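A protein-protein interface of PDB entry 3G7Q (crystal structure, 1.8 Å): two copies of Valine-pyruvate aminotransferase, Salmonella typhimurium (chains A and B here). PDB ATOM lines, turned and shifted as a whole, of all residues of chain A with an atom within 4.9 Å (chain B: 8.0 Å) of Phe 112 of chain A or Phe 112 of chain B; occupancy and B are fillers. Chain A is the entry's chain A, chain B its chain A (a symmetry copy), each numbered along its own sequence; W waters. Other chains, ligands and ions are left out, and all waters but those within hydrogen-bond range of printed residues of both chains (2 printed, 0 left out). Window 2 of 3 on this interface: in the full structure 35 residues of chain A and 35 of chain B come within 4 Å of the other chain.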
ATOM      1  N   GLN A 108       6.928  32.983  -0.966  1.00  0.00           N
ATOM      2  CA  GLN A 108       6.404  31.640  -1.025  1.00  0.00           C
ATOM      3  C   GLN A 108       7.134  30.738  -2.023  1.00  0.00           C
ATOM      4  O   GLN A 108       7.363  29.561  -1.729  1.00  0.00           O
ATOM      5  CB  GLN A 108       4.907  31.718  -1.299  1.00  0.00           C
ATOM      6  CG  GLN A 108       4.181  30.427  -1.026  1.00  0.00           C
ATOM      7  CD  GLN A 108       2.701  30.620  -0.681  1.00  0.00           C
ATOM      8  OE1 GLN A 108       2.197  31.744  -0.609  1.00  0.00           O
ATOM      9  NE2 GLN A 108       2.008  29.512  -0.445  1.00  0.00           N
ATOM     10  N   SER A 109       7.506  31.269  -3.191  1.00  0.00           N
ATOM     11  CA  SER A 109       8.296  30.495  -4.148  1.00  0.00           C
ATOM     12  C   SER A 109       9.711  30.268  -3.588  1.00  0.00           C
ATOM     13  O   SER A 109      10.341  29.240  -3.829  1.00  0.00           O
ATOM     14  CB  SER A 109       8.371  31.210  -5.494  1.00  0.00           C
ATOM     15  OG  SER A 109       8.906  32.515  -5.322  1.00  0.00           O
ATOM     16  N   ALA A 110      10.230  31.261  -2.876  1.00  0.00           N
ATOM     17  CA  ALA A 110      11.520  31.112  -2.209  1.00  0.00           C
ATOM     18  C   ALA A 110      11.519  29.870  -1.302  1.00  0.00           C
ATOM     19  O   ALA A 110      12.407  29.033  -1.404  1.00  0.00           O
ATOM     20  CB  ALA A 110      11.835  32.358  -1.411  1.00  0.00           C
ATOM     21  N   PHE A 111      10.509  29.729  -0.445  1.00  0.00           N
ATOM     22  CA  PHE A 111      10.481  28.571   0.465  1.00  0.00           C
ATOM     23  C   PHE A 111      10.260  27.237  -0.244  1.00  0.00           C
ATOM     24  O   PHE A 111      10.820  26.214   0.170  1.00  0.00           O
ATOM     25  CB  PHE A 111       9.522  28.820   1.625  1.00  0.00           C
ATOM     26  CG  PHE A 111      10.071  29.817   2.590  1.00  0.00           C
ATOM     27  CD1 PHE A 111      10.977  29.418   3.563  1.00  0.00           C
ATOM     28  CD2 PHE A 111       9.781  31.164   2.467  1.00  0.00           C
ATOM     29  CE1 PHE A 111      11.524  30.339   4.427  1.00  0.00           C
ATOM     30  CE2 PHE A 111      10.328  32.081   3.316  1.00  0.00           C
ATOM     31  CZ  PHE A 111      11.209  31.663   4.299  1.00  0.00           C
ATOM     32  N   PHE A 112       9.493  27.249  -1.337  1.00  0.00           N
ATOM     33  CA  PHE A 112       9.317  26.056  -2.132  1.00  0.00           C
ATOM     34  C   PHE A 112      10.668  25.540  -2.612  1.00  0.00           C
ATOM     35  O   PHE A 112      10.934  24.338  -2.568  1.00  0.00           O
ATOM     36  CB  PHE A 112       8.390  26.332  -3.329  1.00  0.00           C
ATOM     37  CG  PHE A 112       8.137  25.132  -4.170  1.00  0.00           C
ATOM     38  CD1 PHE A 112       7.281  24.128  -3.726  1.00  0.00           C
ATOM     39  CD2 PHE A 112       8.758  24.983  -5.397  1.00  0.00           C
ATOM     40  CE1 PHE A 112       7.054  23.002  -4.498  1.00  0.00           C
ATOM     41  CE2 PHE A 112       8.535  23.877  -6.165  1.00  0.00           C
ATOM     42  CZ  PHE A 112       7.687  22.880  -5.725  1.00  0.00           C
ATOM     43  N   TYR A 113      11.531  26.435  -3.089  1.00  0.00           N
ATOM     44  CA  TYR A 113      12.873  26.009  -3.500  1.00  0.00           C
ATOM     45  C   TYR A 113      13.688  25.481  -2.314  1.00  0.00           C
ATOM     46  O   TYR A 113      14.301  24.421  -2.398  1.00  0.00           O
ATOM     47  CB  TYR A 113      13.675  27.139  -4.168  1.00  0.00           C
ATOM     48  CG  TYR A 113      13.094  27.631  -5.474  1.00  0.00           C
ATOM     49  CD1 TYR A 113      12.810  26.740  -6.507  1.00  0.00           C
ATOM     50  CD2 TYR A 113      12.880  28.984  -5.705  1.00  0.00           C
ATOM     51  CE1 TYR A 113      12.274  27.178  -7.713  1.00  0.00           C
ATOM     52  CE2 TYR A 113      12.355  29.434  -6.918  1.00  0.00           C
ATOM     53  CZ  TYR A 113      12.046  28.525  -7.908  1.00  0.00           C
ATOM     54  OH  TYR A 113      11.522  28.958  -9.108  1.00  0.00           O
ATOM     55  N   LEU A 114      13.681  26.211  -1.212  1.00  0.00           N
ATOM     56  CA  LEU A 114      14.480  25.797  -0.055  1.00  0.00           C
ATOM     57  C   LEU A 114      14.026  24.446   0.467  1.00  0.00           C
ATOM     58  O   LEU A 114      14.863  23.570   0.680  1.00  0.00           O
ATOM     59  CB  LEU A 114      14.444  26.875   1.042  1.00  0.00           C
ATOM     60  CG  LEU A 114      15.037  28.230   0.609  1.00  0.00           C
ATOM     61  CD1 LEU A 114      14.805  29.274   1.703  1.00  0.00           C
ATOM     62  CD2 LEU A 114      16.509  28.087   0.234  1.00  0.00           C
ATOM     63  N   PHE A 115      12.713  24.253   0.606  1.00  0.00           N
ATOM     64  CA  PHE A 115      12.178  22.975   1.090  1.00  0.00           C
ATOM     65  C   PHE A 115      12.622  21.840   0.180  1.00  0.00           C
ATOM     66  O   PHE A 115      13.059  20.789   0.652  1.00  0.00           O
ATOM     67  CB  PHE A 115      10.639  22.993   1.238  1.00  0.00           C
ATOM     68  CG  PHE A 115      10.104  24.070   2.186  1.00  0.00           C
ATOM     69  CD1 PHE A 115      10.859  24.559   3.255  1.00  0.00           C
ATOM     70  CD2 PHE A 115       8.798  24.533   2.048  1.00  0.00           C
ATOM     71  CE1 PHE A 115      10.340  25.531   4.123  1.00  0.00           C
ATOM     72  CE2 PHE A 115       8.284  25.483   2.913  1.00  0.00           C
ATOM     73  CZ  PHE A 115       9.058  25.981   3.955  1.00  0.00           C
ATOM     74  N   ASN A 116      12.545  22.057  -1.127  1.00  0.00           N
ATOM     75  CA  ASN A 116      13.026  21.067  -2.085  1.00  0.00           C
ATOM     76  C   ASN A 116      14.518  20.812  -2.023  1.00  0.00           C
ATOM     77  O   ASN A 116      14.962  19.700  -2.261  1.00  0.00           O
ATOM     78  CB  ASN A 116      12.669  21.472  -3.520  1.00  0.00           C
ATOM     79  CG  ASN A 116      11.257  21.103  -3.879  1.00  0.00           C
ATOM     80  OD1 ASN A 116      10.967  19.931  -4.129  1.00  0.00           O
ATOM     81  ND2 ASN A 116      10.366  22.092  -3.915  1.00  0.00           N
ATOM     82  N   ILE A 278      11.635  25.565 -12.923  1.00  0.00           N
ATOM     83  CA  ILE A 278      10.247  25.897 -12.549  1.00  0.00           C
ATOM     84  C   ILE A 278       9.877  27.326 -13.009  1.00  0.00           C
ATOM     85  O   ILE A 278       8.693  27.643 -13.191  1.00  0.00           O
ATOM     86  CB  ILE A 278       9.991  25.729 -11.041  1.00  0.00           C
ATOM     87  N   GLY B 106       4.318  32.484 -16.093  1.00  0.00           N
ATOM     88  CA  GLY B 106       4.790  32.239 -17.448  1.00  0.00           C
ATOM     89  C   GLY B 106       4.541  30.821 -17.916  1.00  0.00           C
ATOM     90  O   GLY B 106       4.007  29.985 -17.181  1.00  0.00           O
ATOM     91  N   SER B 107       4.961  30.564 -19.149  1.00  0.00           N
ATOM     92  CA  SER B 107       4.813  29.260 -19.789  1.00  0.00           C
ATOM     93  C   SER B 107       5.432  28.130 -18.998  1.00  0.00           C
ATOM     94  O   SER B 107       4.821  27.080 -18.800  1.00  0.00           O
ATOM     95  CB  SER B 107       5.459  29.284 -21.179  1.00  0.00           C
ATOM     96  OG  SER B 107       4.750  30.143 -22.071  1.00  0.00           O
ATOM     97  N   GLN B 108       6.636  28.358 -18.510  1.00  0.00           N
ATOM     98  CA  GLN B 108       7.369  27.320 -17.827  1.00  0.00           C
ATOM     99  C   GLN B 108       6.753  26.913 -16.486  1.00  0.00           C
ATOM    100  O   GLN B 108       6.731  25.723 -16.159  1.00  0.00           O
ATOM    101  CB  GLN B 108       8.820  27.764 -17.690  1.00  0.00           C
ATOM    102  CG  GLN B 108       9.757  26.641 -17.330  1.00  0.00           C
ATOM    103  CD  GLN B 108      11.199  26.880 -17.788  1.00  0.00           C
ATOM    104  OE1 GLN B 108      11.517  27.892 -18.419  1.00  0.00           O
ATOM    105  NE2 GLN B 108      12.073  25.926 -17.484  1.00  0.00           N
ATOM    106  N   SER B 109       6.250  27.879 -15.709  1.00  0.00           N
ATOM    107  CA  SER B 109       5.557  27.552 -14.464  1.00  0.00           C
ATOM    108  C   SER B 109       4.222  26.854 -14.782  1.00  0.00           C
ATOM    109  O   SER B 109       3.759  25.986 -14.044  1.00  0.00           O
ATOM    110  CB  SER B 109       5.309  28.808 -13.635  1.00  0.00           C
ATOM    111  OG  SER B 109       4.576  29.758 -14.398  1.00  0.00           O
ATOM    112  N   ALA B 110       3.580  27.274 -15.864  1.00  0.00           N
ATOM    113  CA  ALA B 110       2.360  26.612 -16.319  1.00  0.00           C
ATOM    114  C   ALA B 110       2.602  25.104 -16.505  1.00  0.00           C
ATOM    115  O   ALA B 110       1.859  24.292 -15.971  1.00  0.00           O
ATOM    116  CB  ALA B 110       1.882  27.241 -17.608  1.00  0.00           C
ATOM    117  N   PHE B 111       3.658  24.731 -17.227  1.00  0.00           N
ATOM    118  CA  PHE B 111       3.912  23.299 -17.459  1.00  0.00           C
ATOM    119  C   PHE B 111       4.317  22.535 -16.199  1.00  0.00           C
ATOM    120  O   PHE B 111       3.948  21.364 -16.038  1.00  0.00           O
ATOM    121  CB  PHE B 111       4.867  23.103 -18.632  1.00  0.00           C
ATOM    122  CG  PHE B 111       4.205  23.400 -19.936  1.00  0.00           C
ATOM    123  CD1 PHE B 111       3.418  22.436 -20.552  1.00  0.00           C
ATOM    124  CD2 PHE B 111       4.266  24.662 -20.497  1.00  0.00           C
ATOM    125  CE1 PHE B 111       2.765  22.716 -21.731  1.00  0.00           C
ATOM    126  CE2 PHE B 111       3.613  24.947 -21.661  1.00  0.00           C
ATOM    127  CZ  PHE B 111       2.855  23.966 -22.278  1.00  0.00           C
ATOM    128  N   PHE B 112       5.024  23.202 -15.284  1.00  0.00           N
ATOM    129  CA  PHE B 112       5.358  22.594 -14.017  1.00  0.00           C
ATOM    130  C   PHE B 112       4.089  22.166 -13.289  1.00  0.00           C
ATOM    131  O   PHE B 112       4.024  21.070 -12.731  1.00  0.00           O
ATOM    132  CB  PHE B 112       6.175  23.565 -13.147  1.00  0.00           C
ATOM    133  CG  PHE B 112       6.584  22.986 -11.841  1.00  0.00           C
ATOM    134  CD1 PHE B 112       7.610  22.047 -11.775  1.00  0.00           C
ATOM    135  CD2 PHE B 112       5.944  23.355 -10.671  1.00  0.00           C
ATOM    136  CE1 PHE B 112       7.984  21.494 -10.562  1.00  0.00           C
ATOM    137  CE2 PHE B 112       6.312  22.816  -9.472  1.00  0.00           C
ATOM    138  CZ  PHE B 112       7.328  21.883  -9.405  1.00  0.00           C
ATOM    139  N   TYR B 113       3.072  23.026 -13.273  1.00  0.00           N
ATOM    140  CA  TYR B 113       1.802  22.642 -12.650  1.00  0.00           C
ATOM    141  C   TYR B 113       1.135  21.480 -13.393  1.00  0.00           C
ATOM    142  O   TYR B 113       0.700  20.510 -12.776  1.00  0.00           O
ATOM    143  CB  TYR B 113       0.799  23.807 -12.583  1.00  0.00           C
ATOM    144  CG  TYR B 113       1.236  24.959 -11.707  1.00  0.00           C
ATOM    145  CD1 TYR B 113       1.616  24.744 -10.386  1.00  0.00           C
ATOM    146  CD2 TYR B 113       1.217  26.268 -12.175  1.00  0.00           C
ATOM    147  CE1 TYR B 113       2.023  25.795  -9.569  1.00  0.00           C
ATOM    148  CE2 TYR B 113       1.610  27.330 -11.358  1.00  0.00           C
ATOM    149  CZ  TYR B 113       2.020  27.082 -10.065  1.00  0.00           C
ATOM    150  OH  TYR B 113       2.415  28.123  -9.251  1.00  0.00           O
ATOM    151  N   LEU B 114       1.070  21.569 -14.710  1.00  0.00           N
ATOM    152  CA  LEU B 114       0.399  20.521 -15.483  1.00  0.00           C
ATOM    153  C   LEU B 114       1.089  19.181 -15.300  1.00  0.00           C
ATOM    154  O   LEU B 114       0.415  18.190 -15.023  1.00  0.00           O
ATOM    155  CB  LEU B 114       0.306  20.918 -16.966  1.00  0.00           C
ATOM    156  CG  LEU B 114      -0.517  22.195 -17.223  1.00  0.00           C
ATOM    157  CD1 LEU B 114      -0.412  22.595 -18.697  1.00  0.00           C
ATOM    158  CD2 LEU B 114      -1.961  22.015 -16.764  1.00  0.00           C
ATOM    159  N   PHE B 115       2.420  19.161 -15.384  1.00  0.00           N
ATOM    160  CA  PHE B 115       3.176  17.916 -15.206  1.00  0.00           C
ATOM    161  C   PHE B 115       2.884  17.313 -13.840  1.00  0.00           C
ATOM    162  O   PHE B 115       2.644  16.110 -13.721  1.00  0.00           O
ATOM    163  CB  PHE B 115       4.697  18.110 -15.409  1.00  0.00           C
ATOM    164  CG  PHE B 115       5.090  18.658 -16.783  1.00  0.00           C
ATOM    165  CD1 PHE B 115       4.311  18.435 -17.922  1.00  0.00           C
ATOM    166  CD2 PHE B 115       6.295  19.336 -16.944  1.00  0.00           C
ATOM    167  CE1 PHE B 115       4.702  18.931 -19.174  1.00  0.00           C
ATOM    168  CE2 PHE B 115       6.684  19.813 -18.184  1.00  0.00           C
ATOM    169  CZ  PHE B 115       5.885  19.607 -19.302  1.00  0.00           C
ATOM    170  N   ASN B 116       2.869  18.149 -12.809  1.00  0.00           N
ATOM    171  CA  ASN B 116       2.515  17.687 -11.470  1.00  0.00           C
ATOM    172  C   ASN B 116       1.089  17.195 -11.337  1.00  0.00           C
ATOM    173  O   ASN B 116       0.821  16.285 -10.569  1.00  0.00           O
ATOM    174  CB  ASN B 116       2.740  18.792 -10.432  1.00  0.00           C
ATOM    175  CG  ASN B 116       4.176  18.879  -9.999  1.00  0.00           C
ATOM    176  OD1 ASN B 116       4.642  18.043  -9.222  1.00  0.00           O
ATOM    177  ND2 ASN B 116       4.892  19.891 -10.487  1.00  0.00           N
ATOM    178  N   LEU B 117       0.170  17.806 -12.073  1.00  0.00           N
ATOM    179  CA  LEU B 117      -1.241  17.447 -11.971  1.00  0.00           C
ATOM    180  C   LEU B 117      -1.579  16.143 -12.712  1.00  0.00           C
ATOM    181  O   LEU B 117      -2.391  15.359 -12.237  1.00  0.00           O
ATOM    182  CB  LEU B 117      -2.082  18.607 -12.516  1.00  0.00           C
ATOM    183  CG  LEU B 117      -3.581  18.647 -12.273  1.00  0.00           C
ATOM    184  CD1 LEU B 117      -3.874  18.751 -10.786  1.00  0.00           C
ATOM    185  CD2 LEU B 117      -4.204  19.825 -13.022  1.00  0.00           C
ATOM    186  N   PHE B 118      -0.946  15.904 -13.858  1.00  0.00           N
ATOM    187  CA  PHE B 118      -1.264  14.733 -14.680  1.00  0.00           C
ATOM    188  C   PHE B 118      -0.180  13.649 -14.821  1.00  0.00           C
ATOM    189  O   PHE B 118      -0.499  12.552 -15.267  1.00  0.00           O
ATOM    190  CB  PHE B 118      -1.683  15.193 -16.093  1.00  0.00           C
ATOM    191  CG  PHE B 118      -2.918  16.056 -16.111  1.00  0.00           C
ATOM    192  CD1 PHE B 118      -4.173  15.489 -16.019  1.00  0.00           C
ATOM    193  CD2 PHE B 118      -2.818  17.428 -16.244  1.00  0.00           C
ATOM    194  CE1 PHE B 118      -5.316  16.272 -16.030  1.00  0.00           C
ATOM    195  CE2 PHE B 118      -3.939  18.216 -16.262  1.00  0.00           C
ATOM    196  CZ  PHE B 118      -5.197  17.637 -16.155  1.00  0.00           C
ATOM    197  N   ALA B 119       1.074  13.950 -14.493  1.00  0.00           N
ATOM    198  CA  ALA B 119       2.169  12.989 -14.630  1.00  0.00           C
ATOM    199  C   ALA B 119       2.756  12.678 -13.249  1.00  0.00           C
ATOM    200  O   ALA B 119       2.373  13.288 -12.254  1.00  0.00           O
ATOM    201  CB  ALA B 119       3.244  13.516 -15.567  1.00  0.00           C
ATOM    202  N   ILE B 139       9.746  22.415 -24.232  1.00  0.00           N
ATOM    203  CA  ILE B 139       9.554  22.157 -22.776  1.00  0.00           C
ATOM    204  C   ILE B 139      10.371  20.944 -22.261  1.00  0.00           C
ATOM    205  O   ILE B 139      10.887  20.958 -21.123  1.00  0.00           O
ATOM    206  CB  ILE B 139       8.044  22.083 -22.373  1.00  0.00           C
ATOM    207  CG1 ILE B 139       7.912  22.124 -20.836  1.00  0.00           C
ATOM    208  CG2 ILE B 139       7.362  20.874 -23.000  1.00  0.00           C
ATOM    209  CD1 ILE B 139       8.524  23.391 -20.186  1.00  0.00           C
ATOM    210  N   ASP B 143      12.963  21.667 -19.186  1.00  0.00           N
ATOM    211  CA  ASP B 143      12.851  20.908 -17.940  1.00  0.00           C
ATOM    212  C   ASP B 143      13.669  19.616 -17.962  1.00  0.00           C
ATOM    213  O   ASP B 143      14.866  19.642 -18.257  1.00  0.00           O
ATOM    214  CB  ASP B 143      11.386  20.593 -17.673  1.00  0.00           C
ATOM    215  CG  ASP B 143      10.560  21.843 -17.422  1.00  0.00           C
ATOM    216  OD1 ASP B 143      11.028  22.961 -17.730  1.00  0.00           O
ATOM    217  OD2 ASP B 143       9.433  21.703 -16.909  1.00  0.00           O
ATOM    218  N   ILE B 261      -3.595  29.950 -18.784  1.00  0.00           N
ATOM    219  CA  ILE B 261      -4.001  28.570 -19.051  1.00  0.00           C
ATOM    220  C   ILE B 261      -5.494  28.566 -19.271  1.00  0.00           C
ATOM    221  O   ILE B 261      -6.257  29.120 -18.463  1.00  0.00           O
ATOM    222  CB  ILE B 261      -3.678  27.606 -17.906  1.00  0.00           C
ATOM    223  CG1 ILE B 261      -2.169  27.508 -17.682  1.00  0.00           C
ATOM    224  CG2 ILE B 261      -4.239  26.217 -18.175  1.00  0.00           C
ATOM    225  CD1 ILE B 261      -1.824  26.787 -16.362  1.00  0.00           C
ATOM    226  N   MET B 274      -2.564  24.678  -6.486  1.00  0.00           N
ATOM    227  CA  MET B 274      -1.104  24.652  -6.630  1.00  0.00           C
ATOM    228  C   MET B 274      -0.448  26.044  -6.632  1.00  0.00           C
ATOM    229  O   MET B 274       0.473  26.292  -5.849  1.00  0.00           O
ATOM    230  CB  MET B 274      -0.716  23.866  -7.887  1.00  0.00           C
ATOM    231  CG  MET B 274      -0.898  22.367  -7.714  1.00  0.00           C
ATOM    232  SD  MET B 274      -0.503  21.383  -9.332  1.00  0.00           S
ATOM    233  CE  MET B 274      -2.191  21.632 -10.176  1.00  0.00           C
ATOM    234  N   ILE B 277      -0.145  27.541  -3.368  1.00  0.00           N
ATOM    235  CA  ILE B 277       0.941  27.010  -2.534  1.00  0.00           C
ATOM    236  C   ILE B 277       2.352  27.376  -3.015  1.00  0.00           C
ATOM    237  O   ILE B 277       3.139  27.908  -2.230  1.00  0.00           O
ATOM    238  CB  ILE B 277       0.885  25.481  -2.432  1.00  0.00           C
ATOM    239  CG1 ILE B 277      -0.453  25.016  -1.865  1.00  0.00           C
ATOM    240  CG2 ILE B 277       2.015  24.980  -1.545  1.00  0.00           C
ATOM    241  CD1 ILE B 277      -0.547  23.505  -1.754  1.00  0.00           C
ATOM    242  N   ILE B 278       2.693  27.051  -4.266  1.00  0.00           N
ATOM    243  CA  ILE B 278       4.023  27.380  -4.812  1.00  0.00           C
ATOM    244  C   ILE B 278       4.135  28.889  -5.124  1.00  0.00           C
ATOM    245  O   ILE B 278       5.243  29.443  -5.170  1.00  0.00           O
ATOM    246  CB  ILE B 278       4.367  26.543  -6.057  1.00  0.00           C
ATOM    247  N   SER B 279       2.986  29.535  -5.351  1.00  0.00           N
ATOM    248  CA  SER B 279       2.894  30.990  -5.540  1.00  0.00           C
ATOM    249  C   SER B 279       3.699  31.508  -6.704  1.00  0.00           C
ATOM    250  O   SER B 279       4.642  32.284  -6.526  1.00  0.00           O
ATOM    251  CB  SER B 279       3.298  31.732  -4.246  1.00  0.00           C
ATOM    252  N   LEU B 280       3.319  31.059  -7.894  1.00  0.00           N
ATOM    253  CA  LEU B 280       3.919  31.536  -9.105  1.00  0.00           C
ATOM    254  C   LEU B 280       2.814  32.234  -9.926  1.00  0.00           C
ATOM    255  O   LEU B 280       2.600  31.909 -11.106  1.00  0.00           O
ATOM    256  CB  LEU B 280       4.579  30.379  -9.859  1.00  0.00           C
HETATM  257  O   HOH W   1       6.123  33.619  -4.403  1.00  0.00           O
HETATM  258  O   HOH W   2       5.853  27.612  -0.915  1.00  0.00           O
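The side-chain amide nitrogen (NE2) of Gln 108 of chain A is in hydrogen-bond range of the backbone carbonyl oxygen (O) of Ile 277 of chain B, 2.7 Å away.
The side-chain hydroxyl (OG) of Ser 109 of chain B is in hydrogen-bond range of the backbone carbonyl oxygen (O) of Gly 106 of chain B. The side-chain amide nitrogen (ND2) of Asn 116 of chain A lies within hydrogen-bond range of the backbone carbonyl oxygen (O) of Phe 112 of chain A, 2.7 Å away. The side-chain amide nitrogen of Gln 108 of chain B lies within hydrogen-bond range of the side-chain carboxylate of Asp 143 of chain B. The backbone carbonyl oxygen (O) of Phe 112 of chain B lies within hydrogen-bond range of the side-chain amide nitrogen (ND2) of Asn 116 of chain B.
Among the printed residues, pairs that only touch across the chains: Gln 108 of chain A with Ser 279 of chain B (3.4 Å), Ile 278 of chain A with Ser 109 of chain B (3.4 Å), Ser 109 of chain A with Ile 278 of chain B (3.4 Å), Phe 112 of chain A with Phe 112 of chain B (3.8 Å), Ile 278 of chain A with Gln 108 of chain B (3.9 Å) and Gln 108 of chain A with Ile 278 of chain B (3.9 Å).
Phe 112 of chain A touches just one residue of chain B: Phe 112. Tyr 113 of chain A touches none of the printed residues of chain B. Printed residues of chain B within 4 Å of Ile 278 of chain A: Gln 108 (3.9 Å) and Ser 109 (3.4 Å). Printed residues of chain A within 4 Å of Ser 109 of chain B: Ile 278 (3.4 Å). Phe 112 of chain B touches one residue of chain A. Of the printed residues of chain A, Ile 277 of chain B touches Gln 108 (2.7 Å). Printed residues of chain A within 4 Å of Ile 278 of chain B: Gln 108 (3.9 Å) and Ser 109 (3.4 Å). Of the printed residues of chain A, Ser 279 of chain B touches Gln 108 (3.4 Å).
Hydrophobic or aromatic side chains of chain B that line the printed part of chain A: Phe 112. Of the 10 printed residues of chain A, 4 touch a printed residue of chain B. Hydrophobic or aromatic side chains of chain A within 4 Å of the printed part of chain B: Phe 112. Along chain A the printed residues that touch a printed residue of chain B span positions 108 to 278. Among the printed residues, 7 pairs touch across the chains. Among the printed residues, no Asp or Glu carboxylate lies within 4 Å of a Lys or Arg side-chain nitrogen of the other chain.
Gln 108 of chain A touches Ile 278 of chain B, and with the chains exchanged Ile 278 of chain A touches Gln 108 of chain B. Ser 109 of chain A touches Ile 278 of chain B, and with the chains exchanged Ile 278 of chain A touches Ser 109 of chain B. Phe 112 of chain B touches its own counterpart, Phe 112 of chain A. Positions printed for both chains: 108, 109, 110, 111, 112, 113, 114, 115, 116 and 278. Of the 7 pairs that touch across the chains among the printed residues, 5 have their exchanged pair printed and touching as well.
Water W2 lies within hydrogen-bond range of O of Gln 108 of chain A (2.6 Å) and O of Ile 277 of chain B (3.0 Å). Water W1 lies within hydrogen-bond range of O of Ser 279 of chain B (2.9 Å) and N of Ser 109 of chain A (3.0 Å).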
